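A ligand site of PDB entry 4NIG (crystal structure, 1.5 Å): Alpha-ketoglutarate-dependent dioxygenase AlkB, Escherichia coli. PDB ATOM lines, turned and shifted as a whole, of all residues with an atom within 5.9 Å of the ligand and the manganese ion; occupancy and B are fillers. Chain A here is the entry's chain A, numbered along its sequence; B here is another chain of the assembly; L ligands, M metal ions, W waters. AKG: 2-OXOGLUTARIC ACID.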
ATOM      1  N   MET A  50     -25.191 -29.207  21.767  1.00  0.00           N
ATOM      2  CA  MET A  50     -24.053 -29.958  21.194  1.00  0.00           C
ATOM      3  C   MET A  50     -24.478 -31.111  20.284  1.00  0.00           C
ATOM      4  O   MET A  50     -25.560 -31.679  20.443  1.00  0.00           O
ATOM      5  CB  MET A  50     -23.234 -30.570  22.348  1.00  0.00           C
ATOM      6  CG  MET A  50     -22.553 -29.544  23.211  1.00  0.00           C
ATOM      7  SD  MET A  50     -21.656 -30.181  24.662  1.00  0.00           S
ATOM      8  CE  MET A  50     -20.531 -28.826  24.878  1.00  0.00           C
ATOM      9  N   LEU A 107     -16.505 -32.130  18.321  1.00  0.00           N
ATOM     10  CA  LEU A 107     -17.612 -31.699  19.157  1.00  0.00           C
ATOM     11  C   LEU A 107     -18.034 -30.362  18.562  1.00  0.00           C
ATOM     12  O   LEU A 107     -17.232 -29.447  18.391  1.00  0.00           O
ATOM     13  CB  LEU A 107     -17.136 -31.546  20.635  1.00  0.00           C
ATOM     14  CG  LEU A 107     -18.107 -30.906  21.583  1.00  0.00           C
ATOM     15  CD1 LEU A 107     -19.403 -31.714  21.635  1.00  0.00           C
ATOM     16  CD2 LEU A 107     -17.527 -30.757  22.977  1.00  0.00           C
ATOM     17  N   ASN A 109     -20.533 -27.219  18.975  1.00  0.00           N
ATOM     18  CA  ASN A 109     -21.223 -26.445  20.004  1.00  0.00           C
ATOM     19  C   ASN A 109     -22.064 -25.369  19.273  1.00  0.00           C
ATOM     20  O   ASN A 109     -21.529 -24.712  18.367  1.00  0.00           O
ATOM     21  CB  ASN A 109     -20.238 -25.726  20.907  1.00  0.00           C
ATOM     22  CG  ASN A 109     -19.570 -26.630  21.946  1.00  0.00           C
ATOM     23  OD1 ASN A 109     -18.848 -26.103  22.806  1.00  0.00           O
ATOM     24  ND2 ASN A 109     -19.770 -27.879  21.895  1.00  0.00           N
ATOM     25  N   TYR A 111     -24.119 -21.880  20.396  1.00  0.00           N
ATOM     26  CA  TYR A 111     -24.434 -20.916  21.421  1.00  0.00           C
ATOM     27  C   TYR A 111     -25.554 -19.970  20.966  1.00  0.00           C
ATOM     28  O   TYR A 111     -25.376 -19.264  19.969  1.00  0.00           O
ATOM     29  CB  TYR A 111     -23.196 -20.062  21.782  1.00  0.00           C
ATOM     30  CG  TYR A 111     -21.997 -20.835  22.333  1.00  0.00           C
ATOM     31  CD1 TYR A 111     -21.198 -21.578  21.510  1.00  0.00           C
ATOM     32  CD2 TYR A 111     -21.709 -20.775  23.678  1.00  0.00           C
ATOM     33  CE1 TYR A 111     -20.086 -22.259  22.012  1.00  0.00           C
ATOM     34  CE2 TYR A 111     -20.614 -21.472  24.198  1.00  0.00           C
ATOM     35  CZ  TYR A 111     -19.839 -22.202  23.360  1.00  0.00           C
ATOM     36  OH  TYR A 111     -18.769 -22.906  23.856  1.00  0.00           O
ATOM     37  N   LEU A 117     -20.015 -21.528  28.663  1.00  0.00           N
ATOM     38  CA  LEU A 117     -19.397 -22.756  29.023  1.00  0.00           C
ATOM     39  C   LEU A 117     -18.389 -22.446  30.123  1.00  0.00           C
ATOM     40  O   LEU A 117     -17.357 -21.828  29.864  1.00  0.00           O
ATOM     41  CB  LEU A 117     -18.703 -23.374  27.825  1.00  0.00           C
ATOM     42  CG  LEU A 117     -18.375 -24.841  27.849  1.00  0.00           C
ATOM     43  CD1 LEU A 117     -19.604 -25.706  28.080  1.00  0.00           C
ATOM     44  CD2 LEU A 117     -17.658 -25.222  26.562  1.00  0.00           C
ATOM     45  N   HIS A 120     -13.267 -25.065  32.438  1.00  0.00           N
ATOM     46  CA  HIS A 120     -13.080 -26.513  32.488  1.00  0.00           C
ATOM     47  C   HIS A 120     -11.767 -26.863  31.807  1.00  0.00           C
ATOM     48  O   HIS A 120     -11.144 -26.036  31.140  1.00  0.00           O
ATOM     49  CB  HIS A 120     -14.258 -27.271  31.799  1.00  0.00           C
ATOM     50  CG  HIS A 120     -14.337 -27.055  30.322  1.00  0.00           C
ATOM     51  ND1 HIS A 120     -14.966 -25.963  29.790  1.00  0.00           N
ATOM     52  CD2 HIS A 120     -13.836 -27.768  29.268  1.00  0.00           C
ATOM     53  CE1 HIS A 120     -14.833 -25.994  28.472  1.00  0.00           C
ATOM     54  NE2 HIS A 120     -14.220 -27.098  28.131  1.00  0.00           N
ATOM     55  N   GLN A 121     -11.361 -28.121  31.988  1.00  0.00           N
ATOM     56  CA  GLN A 121     -10.218 -28.711  31.289  1.00  0.00           C
ATOM     57  C   GLN A 121     -10.734 -29.766  30.309  1.00  0.00           C
ATOM     58  O   GLN A 121     -11.687 -30.475  30.637  1.00  0.00           O
ATOM     59  CB  GLN A 121      -9.297 -29.419  32.299  1.00  0.00           C
ATOM     60  CG  GLN A 121      -8.673 -28.526  33.344  1.00  0.00           C
ATOM     61  CD  GLN A 121      -7.904 -29.334  34.395  1.00  0.00           C
ATOM     62  OE1 GLN A 121      -8.480 -30.030  35.244  1.00  0.00           O
ATOM     63  NE2 GLN A 121      -6.611 -29.267  34.304  1.00  0.00           N
ATOM     64  N   ASP A 122     -10.087 -29.875  29.150  1.00  0.00           N
ATOM     65  CA  ASP A 122     -10.389 -30.970  28.213  1.00  0.00           C
ATOM     66  C   ASP A 122      -9.472 -32.109  28.659  1.00  0.00           C
ATOM     67  O   ASP A 122      -8.259 -32.000  28.544  1.00  0.00           O
ATOM     68  CB  ASP A 122     -10.140 -30.546  26.766  1.00  0.00           C
ATOM     69  CG  ASP A 122     -11.367 -29.889  26.108  1.00  0.00           C
ATOM     70  OD1 ASP A 122     -11.972 -29.036  26.768  1.00  0.00           O
ATOM     71  OD2 ASP A 122     -11.744 -30.252  24.910  1.00  0.00           O
ATOM     72  N   ILE A 132      -5.580 -29.681  20.841  1.00  0.00           N
ATOM     73  CA  ILE A 132      -6.969 -29.350  20.664  1.00  0.00           C
ATOM     74  C   ILE A 132      -7.030 -28.246  19.635  1.00  0.00           C
ATOM     75  O   ILE A 132      -6.280 -27.268  19.744  1.00  0.00           O
ATOM     76  CB  ILE A 132      -7.572 -28.845  21.952  1.00  0.00           C
ATOM     77  CG1 ILE A 132      -7.395 -29.914  23.045  1.00  0.00           C
ATOM     78  CG2 ILE A 132      -9.041 -28.471  21.736  1.00  0.00           C
ATOM     79  CD1 ILE A 132      -8.338 -29.784  24.186  1.00  0.00           C
ATOM     80  N   SER A 134      -9.722 -25.591  17.870  1.00  0.00           N
ATOM     81  CA  SER A 134     -11.026 -25.007  18.211  1.00  0.00           C
ATOM     82  C   SER A 134     -11.394 -23.867  17.251  1.00  0.00           C
ATOM     83  O   SER A 134     -10.777 -22.818  17.227  1.00  0.00           O
ATOM     84  CB  SER A 134     -10.947 -24.398  19.621  1.00  0.00           C
ATOM     85  OG  SER A 134     -12.158 -24.197  20.296  1.00  0.00           O
ATOM     86  N   SER A 136     -14.048 -21.072  15.624  1.00  0.00           N
ATOM     87  CA  SER A 136     -15.202 -20.169  15.890  1.00  0.00           C
ATOM     88  C   SER A 136     -15.904 -19.763  14.619  1.00  0.00           C
ATOM     89  O   SER A 136     -15.229 -19.375  13.641  1.00  0.00           O
ATOM     90  CB  SER A 136     -14.814 -18.843  16.493  1.00  0.00           C
ATOM     91  OG  SER A 136     -14.211 -19.079  17.765  1.00  0.00           O
ATOM     92  N   PHE A 143     -13.595 -15.643  25.173  1.00  0.00           N
ATOM     93  CA  PHE A 143     -12.933 -16.878  25.508  1.00  0.00           C
ATOM     94  C   PHE A 143     -11.993 -16.575  26.658  1.00  0.00           C
ATOM     95  O   PHE A 143     -11.234 -15.611  26.602  1.00  0.00           O
ATOM     96  CB  PHE A 143     -12.098 -17.318  24.319  1.00  0.00           C
ATOM     97  CG  PHE A 143     -11.361 -18.642  24.480  1.00  0.00           C
ATOM     98  CD1 PHE A 143     -12.031 -19.849  24.684  1.00  0.00           C
ATOM     99  CD2 PHE A 143      -9.992 -18.683  24.342  1.00  0.00           C
ATOM    100  CE1 PHE A 143     -11.344 -21.039  24.775  1.00  0.00           C
ATOM    101  CE2 PHE A 143      -9.282 -19.872  24.429  1.00  0.00           C
ATOM    102  CZ  PHE A 143      -9.965 -21.042  24.649  1.00  0.00           C
ATOM    103  N   LEU A 159     -13.230 -13.894  20.416  1.00  0.00           N
ATOM    104  CA  LEU A 159     -13.050 -14.803  19.306  1.00  0.00           C
ATOM    105  C   LEU A 159     -14.136 -14.420  18.298  1.00  0.00           C
ATOM    106  O   LEU A 159     -15.317 -14.378  18.660  1.00  0.00           O
ATOM    107  CB  LEU A 159     -13.179 -16.269  19.746  1.00  0.00           C
ATOM    108  CG  LEU A 159     -12.115 -16.810  20.758  1.00  0.00           C
ATOM    109  CD1 LEU A 159     -12.315 -18.283  20.948  1.00  0.00           C
ATOM    110  CD2 LEU A 159     -10.751 -16.489  20.221  1.00  0.00           C
ATOM    111  N   TRP A 167      -4.391 -25.415  21.185  1.00  0.00           N
ATOM    112  CA  TRP A 167      -3.541 -25.602  22.384  1.00  0.00           C
ATOM    113  C   TRP A 167      -3.079 -27.026  22.518  1.00  0.00           C
ATOM    114  O   TRP A 167      -3.657 -27.959  21.993  1.00  0.00           O
ATOM    115  CB  TRP A 167      -4.168 -25.017  23.664  1.00  0.00           C
ATOM    116  CG  TRP A 167      -5.482 -25.548  24.177  1.00  0.00           C
ATOM    117  CD1 TRP A 167      -5.669 -26.363  25.263  1.00  0.00           C
ATOM    118  CD2 TRP A 167      -6.806 -25.187  23.731  1.00  0.00           C
ATOM    119  NE1 TRP A 167      -6.980 -26.567  25.517  1.00  0.00           N
ATOM    120  CE2 TRP A 167      -7.717 -25.879  24.571  1.00  0.00           C
ATOM    121  CE3 TRP A 167      -7.308 -24.395  22.681  1.00  0.00           C
ATOM    122  CZ2 TRP A 167      -9.102 -25.766  24.415  1.00  0.00           C
ATOM    123  CZ3 TRP A 167      -8.684 -24.297  22.524  1.00  0.00           C
ATOM    124  CH2 TRP A 167      -9.558 -24.976  23.383  1.00  0.00           C
ATOM    125  N   HIS A 176     -10.227 -23.377  30.505  1.00  0.00           N
ATOM    126  CA  HIS A 176     -10.703 -22.429  29.530  1.00  0.00           C
ATOM    127  C   HIS A 176     -12.231 -22.484  29.538  1.00  0.00           C
ATOM    128  O   HIS A 176     -12.819 -23.429  30.060  1.00  0.00           O
ATOM    129  CB  HIS A 176     -10.190 -22.773  28.122  1.00  0.00           C
ATOM    130  CG  HIS A 176     -10.565 -24.154  27.700  1.00  0.00           C
ATOM    131  ND1 HIS A 176      -9.897 -25.272  28.132  1.00  0.00           N
ATOM    132  CD2 HIS A 176     -11.559 -24.604  26.901  1.00  0.00           C
ATOM    133  CE1 HIS A 176     -10.476 -26.349  27.672  1.00  0.00           C
ATOM    134  NE2 HIS A 176     -11.473 -25.973  26.892  1.00  0.00           N
ATOM    135  N   GLY A 177     -12.860 -21.480  28.919  1.00  0.00           N
ATOM    136  CA  GLY A 177     -14.318 -21.381  28.869  1.00  0.00           C
ATOM    137  C   GLY A 177     -14.769 -20.239  28.016  1.00  0.00           C
ATOM    138  O   GLY A 177     -13.950 -19.500  27.465  1.00  0.00           O
ATOM    139  N   ILE A 178     -16.091 -20.087  27.927  1.00  0.00           N
ATOM    140  CA  ILE A 178     -16.759 -19.017  27.125  1.00  0.00           C
ATOM    141  C   ILE A 178     -17.739 -18.267  28.040  1.00  0.00           C
ATOM    142  O   ILE A 178     -18.528 -18.864  28.751  1.00  0.00           O
ATOM    143  CB  ILE A 178     -17.492 -19.645  25.919  1.00  0.00           C
ATOM    144  CG1 ILE A 178     -16.474 -20.271  24.955  1.00  0.00           C
ATOM    145  CG2 ILE A 178     -18.440 -18.643  25.207  1.00  0.00           C
ATOM    146  CD1 ILE A 178     -15.717 -19.300  24.079  1.00  0.00           C
ATOM    147  N   ARG A 193     -23.609 -18.521  17.641  1.00  0.00           N
ATOM    148  CA  ARG A 193     -22.235 -18.871  17.379  1.00  0.00           C
ATOM    149  C   ARG A 193     -22.118 -20.402  17.386  1.00  0.00           C
ATOM    150  O   ARG A 193     -22.808 -21.099  18.145  1.00  0.00           O
ATOM    151  CB  ARG A 193     -21.344 -18.296  18.502  1.00  0.00           C
ATOM    152  CG  ARG A 193     -19.917 -18.847  18.617  1.00  0.00           C
ATOM    153  CD  ARG A 193     -19.074 -18.103  19.660  1.00  0.00           C
ATOM    154  NE  ARG A 193     -17.670 -18.491  19.562  1.00  0.00           N
ATOM    155  CZ  ARG A 193     -17.098 -19.477  20.249  1.00  0.00           C
ATOM    156  NH1 ARG A 193     -17.785 -20.152  21.168  1.00  0.00           N
ATOM    157  NH2 ARG A 193     -15.794 -19.723  20.041  1.00  0.00           N
ATOM    158  N   ASN A 195     -19.068 -23.500  17.469  1.00  0.00           N
ATOM    159  CA  ASN A 195     -17.650 -23.867  17.645  1.00  0.00           C
ATOM    160  C   ASN A 195     -17.395 -25.323  17.293  1.00  0.00           C
ATOM    161  O   ASN A 195     -18.195 -26.171  17.607  1.00  0.00           O
ATOM    162  CB  ASN A 195     -17.232 -23.579  19.074  1.00  0.00           C
ATOM    163  CG  ASN A 195     -15.737 -23.659  19.258  1.00  0.00           C
ATOM    164  OD1 ASN A 195     -15.241 -24.657  19.737  1.00  0.00           O
ATOM    165  ND2 ASN A 195     -15.034 -22.627  18.840  1.00  0.00           N
ATOM    166  N   THR A 197     -14.665 -28.300  17.981  1.00  0.00           N
ATOM    167  CA  THR A 197     -13.529 -28.739  18.823  1.00  0.00           C
ATOM    168  C   THR A 197     -13.085 -30.108  18.326  1.00  0.00           C
ATOM    169  O   THR A 197     -13.815 -31.106  18.438  1.00  0.00           O
ATOM    170  CB  THR A 197     -14.015 -28.778  20.245  1.00  0.00           C
ATOM    171  OG1 THR A 197     -14.361 -27.453  20.726  1.00  0.00           O
ATOM    172  CG2 THR A 197     -12.879 -29.284  21.081  1.00  0.00           C
ATOM    173  P   6MA B   8     -16.532 -29.013  34.915  1.00  0.00           P
ATOM    174  OP1 6MA B   8     -16.531 -30.472  34.569  1.00  0.00           O
ATOM    175  OP2 6MA B   8     -15.332 -28.204  34.705  1.00  0.00           O
ATOM    176  O5' 6MA B   8     -17.691 -28.359  33.899  1.00  0.00           O
ATOM    177  C5' 6MA B   8     -17.784 -26.957  33.697  1.00  0.00           C
ATOM    178  C4' 6MA B   8     -18.568 -26.806  32.372  1.00  0.00           C
ATOM    179  O4' 6MA B   8     -17.720 -27.305  31.320  1.00  0.00           O
ATOM    180  C3' 6MA B   8     -19.838 -27.579  32.408  1.00  0.00           C
ATOM    181  O3' 6MA B   8     -20.805 -26.937  31.537  1.00  0.00           O
ATOM    182  C2' 6MA B   8     -19.545 -28.831  31.595  1.00  0.00           C
ATOM    183  C1' 6MA B   8     -18.445 -28.378  30.619  1.00  0.00           C
ATOM    184  N9  6MA B   8     -17.421 -29.395  30.259  1.00  0.00           N
ATOM    185  C8  6MA B   8     -16.617 -30.063  31.149  1.00  0.00           C
ATOM    186  N7  6MA B   8     -15.704 -30.845  30.531  1.00  0.00           N
ATOM    187  C5  6MA B   8     -15.900 -30.649  29.192  1.00  0.00           C
ATOM    188  C6  6MA B   8     -15.251 -31.165  27.985  1.00  0.00           C
ATOM    189  N1  6MA B   8     -15.726 -30.703  26.812  1.00  0.00           N
ATOM    190  C2  6MA B   8     -16.724 -29.768  26.724  1.00  0.00           C
ATOM    191  N3  6MA B   8     -17.352 -29.267  27.809  1.00  0.00           N
ATOM    192  C4  6MA B   8     -16.970 -29.671  29.044  1.00  0.00           C
ATOM    193  N6  6MA B   8     -14.244 -32.093  28.139  1.00  0.00           N
ATOM    194  C1  6MA B   8     -13.697 -32.739  26.932  1.00  0.00           C
HETATM  195  C1  AKG L   1     -15.421 -27.194  24.310  1.00  0.00           C
HETATM  196  O1  AKG L   1     -16.432 -27.540  23.621  1.00  0.00           O
HETATM  197  O2  AKG L   1     -14.741 -28.043  24.928  1.00  0.00           O
HETATM  198  C2  AKG L   1     -15.001 -25.811  24.409  1.00  0.00           C
HETATM  199  O5  AKG L   1     -14.203 -25.486  25.255  1.00  0.00           O
HETATM  200  C3  AKG L   1     -15.544 -24.788  23.442  1.00  0.00           C
HETATM  201  C4  AKG L   1     -14.888 -23.424  23.510  1.00  0.00           C
HETATM  202  C5  AKG L   1     -15.472 -22.479  22.454  1.00  0.00           C
HETATM  203  O3  AKG L   1     -16.693 -22.573  22.185  1.00  0.00           O
HETATM  204  O4  AKG L   1     -14.689 -21.664  21.957  1.00  0.00           O
HETATM  205 MN    MN M   1     -13.089 -27.361  26.208  1.00  0.00          MN
HETATM  206  O   HOH W   1     -11.782 -27.542  24.217  1.00  0.00           O
HETATM  207  O   HOH W   2     -16.996 -27.294  20.355  1.00  0.00           O
HETATM  208  O   HOH W   3     -12.766 -26.097  22.319  1.00  0.00           O
HETATM  209  O   HOH W   4     -12.084 -21.757  21.340  1.00  0.00           O
HETATM  210  O   HOH W   5     -14.294 -30.624  24.458  1.00  0.00           O
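The nearest printed residue that does not touch the manganese ion is 6MA 8 of chain B (4.3 Å).
The manganese ion is bound by OD1 of Asp 122, 2.1 Å away.
O2 of the ligand binds the manganese ion, at 2.2 Å.
The manganese ion is bound by a ring nitrogen (NE2) of His 176.
NE2 of His 120 is bound to the manganese ion (2.2 Å).
An oxygen (O5) of the ligand is bound to the manganese ion, at 2.4 Å.
Water W1 binds the manganese ion (2.4 Å).
Water W5 bridges the side-chain carboxylate of Asp 122 (2.6 Å) and N1 of 6MA 8 of chain B (2.8 Å).
Water W4 bridges the side-chain hydroxyl (OG) of Ser 134 (2.7 Å) and an oxygen (O4) of the ligand (2.7 Å).
Water W3 lies within hydrogen-bond range of the side-chain hydroxyl (OG1) of Thr 197 (2.6 Å) and the side-chain hydroxyl (OG) of Ser 134 (2.8 Å).
Water W2 lies within hydrogen-bond range of OG1 of Thr 197, O of Leu 107, O of Asn 195, ND2 of Asn 109 and O1 of the ligand.
N of Thr 197 lies within hydrogen-bond range of O of Leu 107, 2.8 Å away.
O4' of 6MA 8 of chain B lies within hydrogen-bond range of a ring nitrogen (ND1) of His 120.
NH2 of Arg 193 sits close to ND2 of Asn 195 (3.2 Å).
OH of Tyr 111 is in hydrogen-bond range of OD1 of Asn 109, at 3.4 Å.
The backbone NH (N) of Ile 178 is in hydrogen-bond range of the backbone carbonyl oxygen (O) of Leu 117 (2.9 Å).
The side-chain amide oxygen of Asn 195 lies within hydrogen-bond range of the side-chain hydroxyl of Ser 134 (3.2 Å).
The backbone carbonyl oxygen (O) of Asn 109 is in hydrogen-bond range of the backbone NH (N) of Asn 195.
OD1 of Asn 195 sits at hydrogen-bond distance from OG1 of Thr 197, 3.1 Å away.
The guanidinium group (NH1) of Arg 193 is in salt-bridge range of an oxygen (O3) of the ligand, 2.8 Å away.
An oxygen (O3) of the ligand sits at hydrogen-bond distance from the side-chain hydroxyl (OH) of Tyr 111 (2.7 Å).
The side-chain amide oxygen of Asn 109 sits close to an oxygen (O1) of the ligand.
The side-chain amide nitrogen (ND2) of Asn 195 sits at hydrogen-bond distance from an oxygen (O4) of the ligand (3.3 Å).
N1 of 6MA 8 of chain B lies close to an oxygen (O2) of the ligand (3.4 Å).
Residues that only touch the ligand: Leu 107 (3.5 Å), Leu 117 (3.5 Å), Ser 134 (3.9 Å), Ile 178 (3.3 Å) and Thr 197 (3.6 Å).
Hydrophobic or aromatic side chains that line the ligand: Leu 107, Tyr 111, Leu 117, His 120, His 176 and Ile 178.
Within 4 Å of the ligand: Leu 107, Asn 109, Tyr 111, Leu 117, His 120, Asp 122, Ser 134, His 176, Ile 178, Arg 193, Asn 195, Thr 197 and 6MA 8 of chain B.
Along chain A the residues within 4 Å of the ligand span positions 107 to 197.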
